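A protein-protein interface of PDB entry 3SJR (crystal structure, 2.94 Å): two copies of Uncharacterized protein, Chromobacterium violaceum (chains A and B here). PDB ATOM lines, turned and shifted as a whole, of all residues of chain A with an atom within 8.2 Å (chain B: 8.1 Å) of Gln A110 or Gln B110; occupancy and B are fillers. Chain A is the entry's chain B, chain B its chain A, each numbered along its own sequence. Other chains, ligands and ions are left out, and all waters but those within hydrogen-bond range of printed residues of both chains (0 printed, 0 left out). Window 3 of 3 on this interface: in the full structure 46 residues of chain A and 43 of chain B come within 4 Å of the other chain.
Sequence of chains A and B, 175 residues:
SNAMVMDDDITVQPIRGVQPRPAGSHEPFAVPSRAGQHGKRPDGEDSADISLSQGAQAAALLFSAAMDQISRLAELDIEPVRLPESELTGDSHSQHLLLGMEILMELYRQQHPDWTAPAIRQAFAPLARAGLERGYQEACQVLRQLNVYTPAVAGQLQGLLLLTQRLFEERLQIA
The side-chain carboxylate of Glu B106 is in hydrogen-bond range of the side-chain amide nitrogen of Gln B110.
The side-chain carboxylate (OE2) of Glu A106 sits close to the side-chain amide oxygen (OE1) of Gln A110 (2.8 Å).
Among the printed residues, merely in contact across the chains: Leu A76 with Leu B104 (3.8 Å), Leu A76 with Tyr B108 (3.7 Å), Leu A76 with Gln B111 (3.2 Å), Ile A103 with Ile B103 (3.8 Å), Ile A103 with Leu B107 (3.9 Å), Leu A104 with Leu B76 (3.3 Å), Glu A106 with Leu B107 (3.7 Å), Leu A107 with Leu B76 (3.7 Å), Leu A107 with Ile B103 (3.6 Å), Tyr A108 with Leu B76 (3.6 Å), Gln A110 with Gln B110 (3.2 Å) and Gln A111 with Leu B76 (3.8 Å).
Gln A110 touches one residue of chain B.
Gln B110 touches one residue of chain A.
Of the printed residues of chain A, Leu B104 touches Leu A76.
Printed residues of chain A within 4 Å of Leu B107: Ile A103 and Glu A106.
Met A105 touches none of the printed residues of chain B.
His A112 touches none of the printed residues of chain B.
The nearest residue of chain A that does not touch Gln B110 is Glu A106 (4.3 Å).
The nearest printed residue of chain A that does not touch Leu B76 is Met A105 (4.9 Å).
Hydrophobic or aromatic side chains of chain B within 4 Å of the printed part of chain A: Leu B76, Ile B103, Leu B104, Leu B107 and Tyr B108.
Of the 14 printed residues of chain A, 8 touch a printed residue of chain B.
Hydrophobic or aromatic side chains of chain A that line the printed part of chain B: Leu A76, Ile A103, Leu A104 and Leu A107.
Along chain A the printed residues that touch a printed residue of chain B span positions 76 to 111.
Leu A76 touches Leu B104, and with the chains exchanged Leu A104 touches Leu B76.
Leu A76 touches Tyr B108, and with the chains exchanged Tyr A108 touches Leu B76.
Ile B103 touches its own counterpart, Ile A103.
Gln A110 touches its own counterpart, Gln B110.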
ATOM      1  N   LEU A  76      -5.489  13.693  30.768  1.00  0.00           N
ATOM      2  CA  LEU A  76      -5.803  14.652  29.739  1.00  0.00           C
ATOM      3  C   LEU A  76      -4.863  14.438  28.571  1.00  0.00           C
ATOM      4  O   LEU A  76      -3.790  15.024  28.545  1.00  0.00           O
ATOM      5  CB  LEU A  76      -5.607  16.064  30.279  1.00  0.00           C
ATOM      6  CG  LEU A  76      -6.119  16.366  31.679  1.00  0.00           C
ATOM      7  CD1 LEU A  76      -5.517  17.660  32.135  1.00  0.00           C
ATOM      8  CD2 LEU A  76      -7.629  16.455  31.684  1.00  0.00           C
ATOM      9  N   ILE A 103      -3.052  21.745  24.685  1.00  0.00           N
ATOM     10  CA  ILE A 103      -4.092  22.071  25.662  1.00  0.00           C
ATOM     11  C   ILE A 103      -4.644  23.466  25.408  1.00  0.00           C
ATOM     12  O   ILE A 103      -5.852  23.645  25.236  1.00  0.00           O
ATOM     13  CB  ILE A 103      -3.591  21.932  27.126  1.00  0.00           C
ATOM     14  CG1 ILE A 103      -3.529  20.452  27.530  1.00  0.00           C
ATOM     15  CG2 ILE A 103      -4.506  22.685  28.087  1.00  0.00           C
ATOM     16  CD1 ILE A 103      -2.874  20.186  28.880  1.00  0.00           C
ATOM     17  N   LEU A 104      -3.753  24.448  25.354  1.00  0.00           N
ATOM     18  CA  LEU A 104      -4.186  25.824  25.184  1.00  0.00           C
ATOM     19  C   LEU A 104      -5.003  25.977  23.914  1.00  0.00           C
ATOM     20  O   LEU A 104      -6.126  26.463  23.955  1.00  0.00           O
ATOM     21  CB  LEU A 104      -2.996  26.774  25.211  1.00  0.00           C
ATOM     22  CG  LEU A 104      -2.245  26.820  26.545  1.00  0.00           C
ATOM     23  CD1 LEU A 104      -1.097  27.815  26.482  1.00  0.00           C
ATOM     24  CD2 LEU A 104      -3.204  27.157  27.681  1.00  0.00           C
ATOM     25  N   MET A 105      -4.465  25.509  22.794  1.00  0.00           N
ATOM     26  CA  MET A 105      -5.202  25.538  21.538  1.00  0.00           C
ATOM     27  C   MET A 105      -6.574  24.917  21.727  1.00  0.00           C
ATOM     28  O   MET A 105      -7.586  25.510  21.348  1.00  0.00           O
ATOM     29  CB  MET A 105      -4.439  24.804  20.450  1.00  0.00           C
ATOM     30  CG  MET A 105      -5.157  24.759  19.112  1.00  0.00           C
ATOM     31  SD  MET A 105      -3.967  24.277  17.641  1.00  0.00           S
ATOM     32  CE  MET A 105      -3.695  22.380  18.029  1.00  0.00           C
ATOM     33  N   GLU A 106      -6.598  23.731  22.334  1.00  0.00           N
ATOM     34  CA  GLU A 106      -7.833  22.989  22.551  1.00  0.00           C
ATOM     35  C   GLU A 106      -8.845  23.871  23.254  1.00  0.00           C
ATOM     36  O   GLU A 106     -10.030  23.867  22.921  1.00  0.00           O
ATOM     37  CB  GLU A 106      -7.570  21.713  23.357  1.00  0.00           C
ATOM     38  CG  GLU A 106      -8.822  20.923  23.733  1.00  0.00           C
ATOM     39  CD  GLU A 106      -9.805  20.737  22.577  1.00  0.00           C
ATOM     40  OE1 GLU A 106      -9.370  20.450  21.438  1.00  0.00           O
ATOM     41  OE2 GLU A 106     -11.025  20.872  22.821  1.00  0.00           O
ATOM     42  N   LEU A 107      -8.362  24.651  24.205  1.00  0.00           N
ATOM     43  CA  LEU A 107      -9.226  25.545  24.933  1.00  0.00           C
ATOM     44  C   LEU A 107      -9.691  26.697  24.038  1.00  0.00           C
ATOM     45  O   LEU A 107     -10.873  27.030  24.017  1.00  0.00           O
ATOM     46  CB  LEU A 107      -8.484  26.073  26.156  1.00  0.00           C
ATOM     47  CG  LEU A 107      -9.195  25.957  27.495  1.00  0.00           C
ATOM     48  CD1 LEU A 107      -9.056  24.535  28.001  1.00  0.00           C
ATOM     49  CD2 LEU A 107      -8.614  26.939  28.486  1.00  0.00           C
ATOM     50  N   TYR A 108      -8.741  27.283  23.309  1.00  0.00           N
ATOM     51  CA  TYR A 108      -8.976  28.365  22.349  1.00  0.00           C
ATOM     52  C   TYR A 108     -10.023  27.964  21.303  1.00  0.00           C
ATOM     53  O   TYR A 108     -10.878  28.778  20.901  1.00  0.00           O
ATOM     54  CB  TYR A 108      -7.645  28.707  21.682  1.00  0.00           C
ATOM     55  CG  TYR A 108      -7.659  29.820  20.657  1.00  0.00           C
ATOM     56  CD1 TYR A 108      -7.837  31.151  21.032  1.00  0.00           C
ATOM     57  CD2 TYR A 108      -7.432  29.549  19.311  1.00  0.00           C
ATOM     58  CE1 TYR A 108      -7.821  32.183  20.083  1.00  0.00           C
ATOM     59  CE2 TYR A 108      -7.415  30.572  18.353  1.00  0.00           C
ATOM     60  CZ  TYR A 108      -7.608  31.886  18.745  1.00  0.00           C
ATOM     61  OH  TYR A 108      -7.597  32.894  17.796  1.00  0.00           O
ATOM     62  N   ARG A 109      -9.941  26.701  20.872  1.00  0.00           N
ATOM     63  CA  ARG A 109     -10.960  26.085  20.038  1.00  0.00           C
ATOM     64  C   ARG A 109     -12.306  26.343  20.674  1.00  0.00           C
ATOM     65  O   ARG A 109     -13.161  26.971  20.072  1.00  0.00           O
ATOM     66  CB  ARG A 109     -10.716  24.575  19.912  1.00  0.00           C
ATOM     67  CG  ARG A 109     -11.796  23.786  19.156  1.00  0.00           C
ATOM     68  CD  ARG A 109     -11.724  24.086  17.668  1.00  0.00           C
ATOM     69  NE  ARG A 109     -12.824  23.532  16.875  1.00  0.00           N
ATOM     70  CZ  ARG A 109     -14.073  23.995  16.876  1.00  0.00           C
ATOM     71  NH1 ARG A 109     -14.426  25.007  17.661  1.00  0.00           N
ATOM     72  NH2 ARG A 109     -14.980  23.425  16.098  1.00  0.00           N
ATOM     73  N   GLN A 110     -12.461  25.892  21.918  1.00  0.00           N
ATOM     74  CA  GLN A 110     -13.742  25.956  22.618  1.00  0.00           C
ATOM     75  C   GLN A 110     -14.233  27.382  22.792  1.00  0.00           C
ATOM     76  O   GLN A 110     -15.424  27.607  22.921  1.00  0.00           O
ATOM     77  CB  GLN A 110     -13.683  25.233  23.974  1.00  0.00           C
ATOM     78  CG  GLN A 110     -13.172  23.789  23.914  1.00  0.00           C
ATOM     79  CD  GLN A 110     -13.870  22.927  22.856  1.00  0.00           C
ATOM     80  OE1 GLN A 110     -13.222  22.390  21.949  1.00  0.00           O
ATOM     81  NE2 GLN A 110     -15.192  22.794  22.966  1.00  0.00           N
ATOM     82  N   GLN A 111     -13.321  28.342  22.772  1.00  0.00           N
ATOM     83  CA  GLN A 111     -13.699  29.747  22.872  1.00  0.00           C
ATOM     84  C   GLN A 111     -14.222  30.307  21.556  1.00  0.00           C
ATOM     85  O   GLN A 111     -14.686  31.441  21.490  1.00  0.00           O
ATOM     86  CB  GLN A 111     -12.523  30.580  23.366  1.00  0.00           C
ATOM     87  CG  GLN A 111     -12.164  30.275  24.802  1.00  0.00           C
ATOM     88  CD  GLN A 111     -11.871  31.520  25.604  1.00  0.00           C
ATOM     89  OE1 GLN A 111     -11.779  32.630  25.057  1.00  0.00           O
ATOM     90  NE2 GLN A 111     -11.719  31.345  26.916  1.00  0.00           N
ATOM     91  N   HIS A 112     -14.113  29.515  20.501  1.00  0.00           N
ATOM     92  CA  HIS A 112     -14.674  29.880  19.225  1.00  0.00           C
ATOM     93  C   HIS A 112     -15.300  28.638  18.646  1.00  0.00           C
ATOM     94  O   HIS A 112     -14.711  28.005  17.768  1.00  0.00           O
ATOM     95  CB  HIS A 112     -13.592  30.405  18.294  1.00  0.00           C
ATOM     96  CG  HIS A 112     -12.728  31.453  18.911  1.00  0.00           C
ATOM     97  ND1 HIS A 112     -13.215  32.684  19.292  1.00  0.00           N
ATOM     98  CD2 HIS A 112     -11.413  31.452  19.228  1.00  0.00           C
ATOM     99  CE1 HIS A 112     -12.234  33.400  19.810  1.00  0.00           C
ATOM    100  NE2 HIS A 112     -11.130  32.675  19.783  1.00  0.00           N
ATOM    101  N   PRO A 113     -16.490  28.262  19.154  1.00  0.00           N
ATOM    102  CA  PRO A 113     -17.206  27.105  18.617  1.00  0.00           C
ATOM    103  C   PRO A 113     -17.623  27.354  17.174  1.00  0.00           C
ATOM    104  O   PRO A 113     -17.677  26.420  16.380  1.00  0.00           O
ATOM    105  CB  PRO A 113     -18.446  27.016  19.508  1.00  0.00           C
ATOM    106  CG  PRO A 113     -18.640  28.399  20.032  1.00  0.00           C
ATOM    107  CD  PRO A 113     -17.264  28.955  20.202  1.00  0.00           C
ATOM    108  N   ASP A 114     -17.884  28.622  16.858  1.00  0.00           N
ATOM    109  CA  ASP A 114     -18.377  29.068  15.550  1.00  0.00           C
ATOM    110  C   ASP A 114     -17.382  28.914  14.381  1.00  0.00           C
ATOM    111  O   ASP A 114     -17.796  28.586  13.266  1.00  0.00           O
ATOM    112  CB  ASP A 114     -18.886  30.518  15.648  1.00  0.00           C
ATOM    113  CG  ASP A 114     -17.832  31.495  16.203  1.00  0.00           C
ATOM    114  OD1 ASP A 114     -16.877  31.076  16.912  1.00  0.00           O
ATOM    115  OD2 ASP A 114     -17.976  32.707  15.929  1.00  0.00           O
ATOM    116  N   ILE A 120      -9.079  27.988  13.008  1.00  0.00           N
ATOM    117  CA  ILE A 120      -8.456  28.152  14.326  1.00  0.00           C
ATOM    118  C   ILE A 120      -6.959  27.831  14.314  1.00  0.00           C
ATOM    119  O   ILE A 120      -6.169  28.451  15.031  1.00  0.00           O
ATOM    120  CB  ILE A 120      -9.178  27.372  15.479  1.00  0.00           C
ATOM    121  CG1 ILE A 120      -8.837  25.885  15.437  1.00  0.00           C
ATOM    122  CG2 ILE A 120     -10.701  27.609  15.470  1.00  0.00           C
ATOM    123  CD1 ILE A 120      -8.357  25.341  16.764  1.00  0.00           C
ATOM    124  N   LEU B  76      -7.038  33.491  26.482  1.00  0.00           N
ATOM    125  CA  LEU B  76      -7.497  32.408  27.336  1.00  0.00           C
ATOM    126  C   LEU B  76      -7.382  32.839  28.783  1.00  0.00           C
ATOM    127  O   LEU B  76      -8.081  32.306  29.652  1.00  0.00           O
ATOM    128  CB  LEU B  76      -6.679  31.141  27.105  1.00  0.00           C
ATOM    129  CG  LEU B  76      -7.032  30.361  25.841  1.00  0.00           C
ATOM    130  CD1 LEU B  76      -5.986  29.295  25.589  1.00  0.00           C
ATOM    131  CD2 LEU B  76      -8.437  29.753  25.908  1.00  0.00           C
ATOM    132  N   ILE B 103      -7.262  25.769  34.073  1.00  0.00           N
ATOM    133  CA  ILE B 103      -7.301  25.246  32.715  1.00  0.00           C
ATOM    134  C   ILE B 103      -7.426  23.725  32.768  1.00  0.00           C
ATOM    135  O   ILE B 103      -8.300  23.128  32.120  1.00  0.00           O
ATOM    136  CB  ILE B 103      -6.019  25.600  31.920  1.00  0.00           C
ATOM    137  CG1 ILE B 103      -5.612  27.075  32.086  1.00  0.00           C
ATOM    138  CG2 ILE B 103      -6.168  25.190  30.463  1.00  0.00           C
ATOM    139  CD1 ILE B 103      -6.417  28.070  31.289  1.00  0.00           C
ATOM    140  N   LEU B 104      -6.550  23.114  33.560  1.00  0.00           N
ATOM    141  CA  LEU B 104      -6.550  21.673  33.757  1.00  0.00           C
ATOM    142  C   LEU B 104      -7.922  21.170  34.177  1.00  0.00           C
ATOM    143  O   LEU B 104      -8.489  20.296  33.522  1.00  0.00           O
ATOM    144  CB  LEU B 104      -5.463  21.273  34.749  1.00  0.00           C
ATOM    145  CG  LEU B 104      -4.058  21.565  34.213  1.00  0.00           C
ATOM    146  CD1 LEU B 104      -2.993  20.951  35.098  1.00  0.00           C
ATOM    147  CD2 LEU B 104      -3.885  21.079  32.773  1.00  0.00           C
ATOM    148  N   MET B 105      -8.476  21.748  35.233  1.00  0.00           N
ATOM    149  CA  MET B 105      -9.833  21.408  35.606  1.00  0.00           C
ATOM    150  C   MET B 105     -10.812  21.606  34.449  1.00  0.00           C
ATOM    151  O   MET B 105     -11.594  20.703  34.149  1.00  0.00           O
ATOM    152  CB  MET B 105     -10.276  22.227  36.795  1.00  0.00           C
ATOM    153  CG  MET B 105     -11.513  21.696  37.435  1.00  0.00           C
ATOM    154  SD  MET B 105     -11.685  22.493  39.185  1.00  0.00           S
ATOM    155  CE  MET B 105     -11.975  24.357  38.646  1.00  0.00           C
ATOM    156  N   GLU B 106     -10.762  22.777  33.805  1.00  0.00           N
ATOM    157  CA  GLU B 106     -11.730  23.105  32.779  1.00  0.00           C
ATOM    158  C   GLU B 106     -11.734  22.024  31.719  1.00  0.00           C
ATOM    159  O   GLU B 106     -12.797  21.548  31.322  1.00  0.00           O
ATOM    160  CB  GLU B 106     -11.475  24.491  32.163  1.00  0.00           C
ATOM    161  CG  GLU B 106     -12.278  24.799  30.850  1.00  0.00           C
ATOM    162  CD  GLU B 106     -13.820  24.672  30.980  1.00  0.00           C
ATOM    163  OE1 GLU B 106     -14.327  24.295  32.063  1.00  0.00           O
ATOM    164  OE2 GLU B 106     -14.537  24.944  29.982  1.00  0.00           O
ATOM    165  N   LEU B 107     -10.541  21.629  31.284  1.00  0.00           N
ATOM    166  CA  LEU B 107     -10.400  20.609  30.250  1.00  0.00           C
ATOM    167  C   LEU B 107     -10.790  19.221  30.772  1.00  0.00           C
ATOM    168  O   LEU B 107     -11.327  18.397  30.034  1.00  0.00           O
ATOM    169  CB  LEU B 107      -8.981  20.610  29.672  1.00  0.00           C
ATOM    170  CG  LEU B 107      -8.706  19.658  28.499  1.00  0.00           C
ATOM    171  CD1 LEU B 107      -9.452  20.091  27.243  1.00  0.00           C
ATOM    172  CD2 LEU B 107      -7.210  19.494  28.213  1.00  0.00           C
ATOM    173  N   TYR B 108     -10.527  18.964  32.045  1.00  0.00           N
ATOM    174  CA  TYR B 108     -10.961  17.730  32.657  1.00  0.00           C
ATOM    175  C   TYR B 108     -12.475  17.645  32.506  1.00  0.00           C
ATOM    176  O   TYR B 108     -13.009  16.610  32.111  1.00  0.00           O
ATOM    177  CB  TYR B 108     -10.548  17.723  34.121  1.00  0.00           C
ATOM    178  CG  TYR B 108     -10.706  16.409  34.838  1.00  0.00           C
ATOM    179  CD1 TYR B 108      -9.931  15.306  34.495  1.00  0.00           C
ATOM    180  CD2 TYR B 108     -11.597  16.281  35.894  1.00  0.00           C
ATOM    181  CE1 TYR B 108     -10.053  14.095  35.172  1.00  0.00           C
ATOM    182  CE2 TYR B 108     -11.729  15.069  36.584  1.00  0.00           C
ATOM    183  CZ  TYR B 108     -10.956  13.980  36.216  1.00  0.00           C
ATOM    184  OH  TYR B 108     -11.090  12.780  36.886  1.00  0.00           O
ATOM    185  N   ARG B 109     -13.144  18.763  32.795  1.00  0.00           N
ATOM    186  CA  ARG B 109     -14.596  18.887  32.728  1.00  0.00           C
ATOM    187  C   ARG B 109     -15.084  18.508  31.344  1.00  0.00           C
ATOM    188  O   ARG B 109     -15.841  17.556  31.182  1.00  0.00           O
ATOM    189  CB  ARG B 109     -15.015  20.326  33.044  1.00  0.00           C
ATOM    190  CG  ARG B 109     -16.481  20.509  33.421  1.00  0.00           C
ATOM    191  CD  ARG B 109     -16.907  21.990  33.334  1.00  0.00           C
ATOM    192  NE  ARG B 109     -17.833  22.270  32.229  1.00  0.00           N
ATOM    193  CZ  ARG B 109     -17.476  22.634  30.995  1.00  0.00           C
ATOM    194  NH1 ARG B 109     -16.197  22.777  30.667  1.00  0.00           N
ATOM    195  NH2 ARG B 109     -18.412  22.854  30.078  1.00  0.00           N
ATOM    196  N   GLN B 110     -14.628  19.259  30.352  1.00  0.00           N
ATOM    197  CA  GLN B 110     -14.929  18.994  28.956  1.00  0.00           C
ATOM    198  C   GLN B 110     -14.735  17.533  28.568  1.00  0.00           C
ATOM    199  O   GLN B 110     -15.529  16.978  27.821  1.00  0.00           O
ATOM    200  CB  GLN B 110     -14.093  19.911  28.072  1.00  0.00           C
ATOM    201  CG  GLN B 110     -14.697  21.309  27.944  1.00  0.00           C
ATOM    202  CD  GLN B 110     -13.727  22.348  27.407  1.00  0.00           C
ATOM    203  OE1 GLN B 110     -12.891  22.066  26.537  1.00  0.00           O
ATOM    204  NE2 GLN B 110     -13.843  23.568  27.916  1.00  0.00           N
ATOM    205  N   GLN B 111     -13.699  16.909  29.108  1.00  0.00           N
ATOM    206  CA  GLN B 111     -13.414  15.506  28.835  1.00  0.00           C
ATOM    207  C   GLN B 111     -14.300  14.510  29.599  1.00  0.00           C
ATOM    208  O   GLN B 111     -14.183  13.305  29.391  1.00  0.00           O
ATOM    209  CB  GLN B 111     -11.939  15.204  29.103  1.00  0.00           C
ATOM    210  CG  GLN B 111     -10.996  15.698  28.016  1.00  0.00           C
ATOM    211  CD  GLN B 111      -9.545  15.375  28.321  1.00  0.00           C
ATOM    212  OE1 GLN B 111      -9.220  14.852  29.392  1.00  0.00           O
ATOM    213  NE2 GLN B 111      -8.662  15.682  27.375  1.00  0.00           N
ATOM    214  N   HIS B 112     -15.160  15.000  30.488  1.00  0.00           N
ATOM    215  CA  HIS B 112     -16.107  14.133  31.199  1.00  0.00           C
ATOM    216  C   HIS B 112     -17.521  14.719  31.153  1.00  0.00           C
ATOM    217  O   HIS B 112     -18.025  15.203  32.174  1.00  0.00           O
ATOM    218  CB  HIS B 112     -15.681  13.915  32.652  1.00  0.00           C
ATOM    219  CG  HIS B 112     -14.403  13.152  32.805  1.00  0.00           C
ATOM    220  ND1 HIS B 112     -14.332  11.783  32.668  1.00  0.00           N
ATOM    221  CD2 HIS B 112     -13.147  13.565  33.104  1.00  0.00           C
ATOM    222  CE1 HIS B 112     -13.087  11.384  32.867  1.00  0.00           C
ATOM    223  NE2 HIS B 112     -12.349  12.446  33.134  1.00  0.00           N
ATOM    224  N   PRO B 113     -18.175  14.663  29.971  1.00  0.00           N
ATOM    225  CA  PRO B 113     -19.483  15.295  29.785  1.00  0.00           C
ATOM    226  C   PRO B 113     -20.586  14.601  30.585  1.00  0.00           C
ATOM    227  O   PRO B 113     -21.454  15.277  31.146  1.00  0.00           O
ATOM    228  CB  PRO B 113     -19.750  15.137  28.278  1.00  0.00           C
ATOM    229  CG  PRO B 113     -18.492  14.568  27.679  1.00  0.00           C
ATOM    230  CD  PRO B 113     -17.780  13.876  28.788  1.00  0.00           C
ATOM    231  N   ASP B 114     -20.533  13.266  30.638  1.00  0.00           N
ATOM    232  CA  ASP B 114     -21.528  12.443  31.332  1.00  0.00           C
ATOM    233  C   ASP B 114     -21.572  12.694  32.832  1.00  0.00           C
ATOM    234  O   ASP B 114     -22.602  12.501  33.474  1.00  0.00           O
ATOM    235  CB  ASP B 114     -21.246  10.964  31.085  1.00  0.00           C
ATOM    236  CG  ASP B 114     -21.571  10.537  29.671  1.00  0.00           C
ATOM    237  OD1 ASP B 114     -22.677  10.850  29.179  1.00  0.00           O
ATOM    238  OD2 ASP B 114     -20.715   9.871  29.055  1.00  0.00           O
ATOM    239  N   ILE B 120     -17.449  15.977  39.254  1.00  0.00           N
ATOM    240  CA  ILE B 120     -16.286  16.471  38.528  1.00  0.00           C
ATOM    241  C   ILE B 120     -15.317  17.183  39.457  1.00  0.00           C
ATOM    242  O   ILE B 120     -14.118  16.956  39.379  1.00  0.00           O
ATOM    243  CB  ILE B 120     -16.702  17.375  37.385  1.00  0.00           C
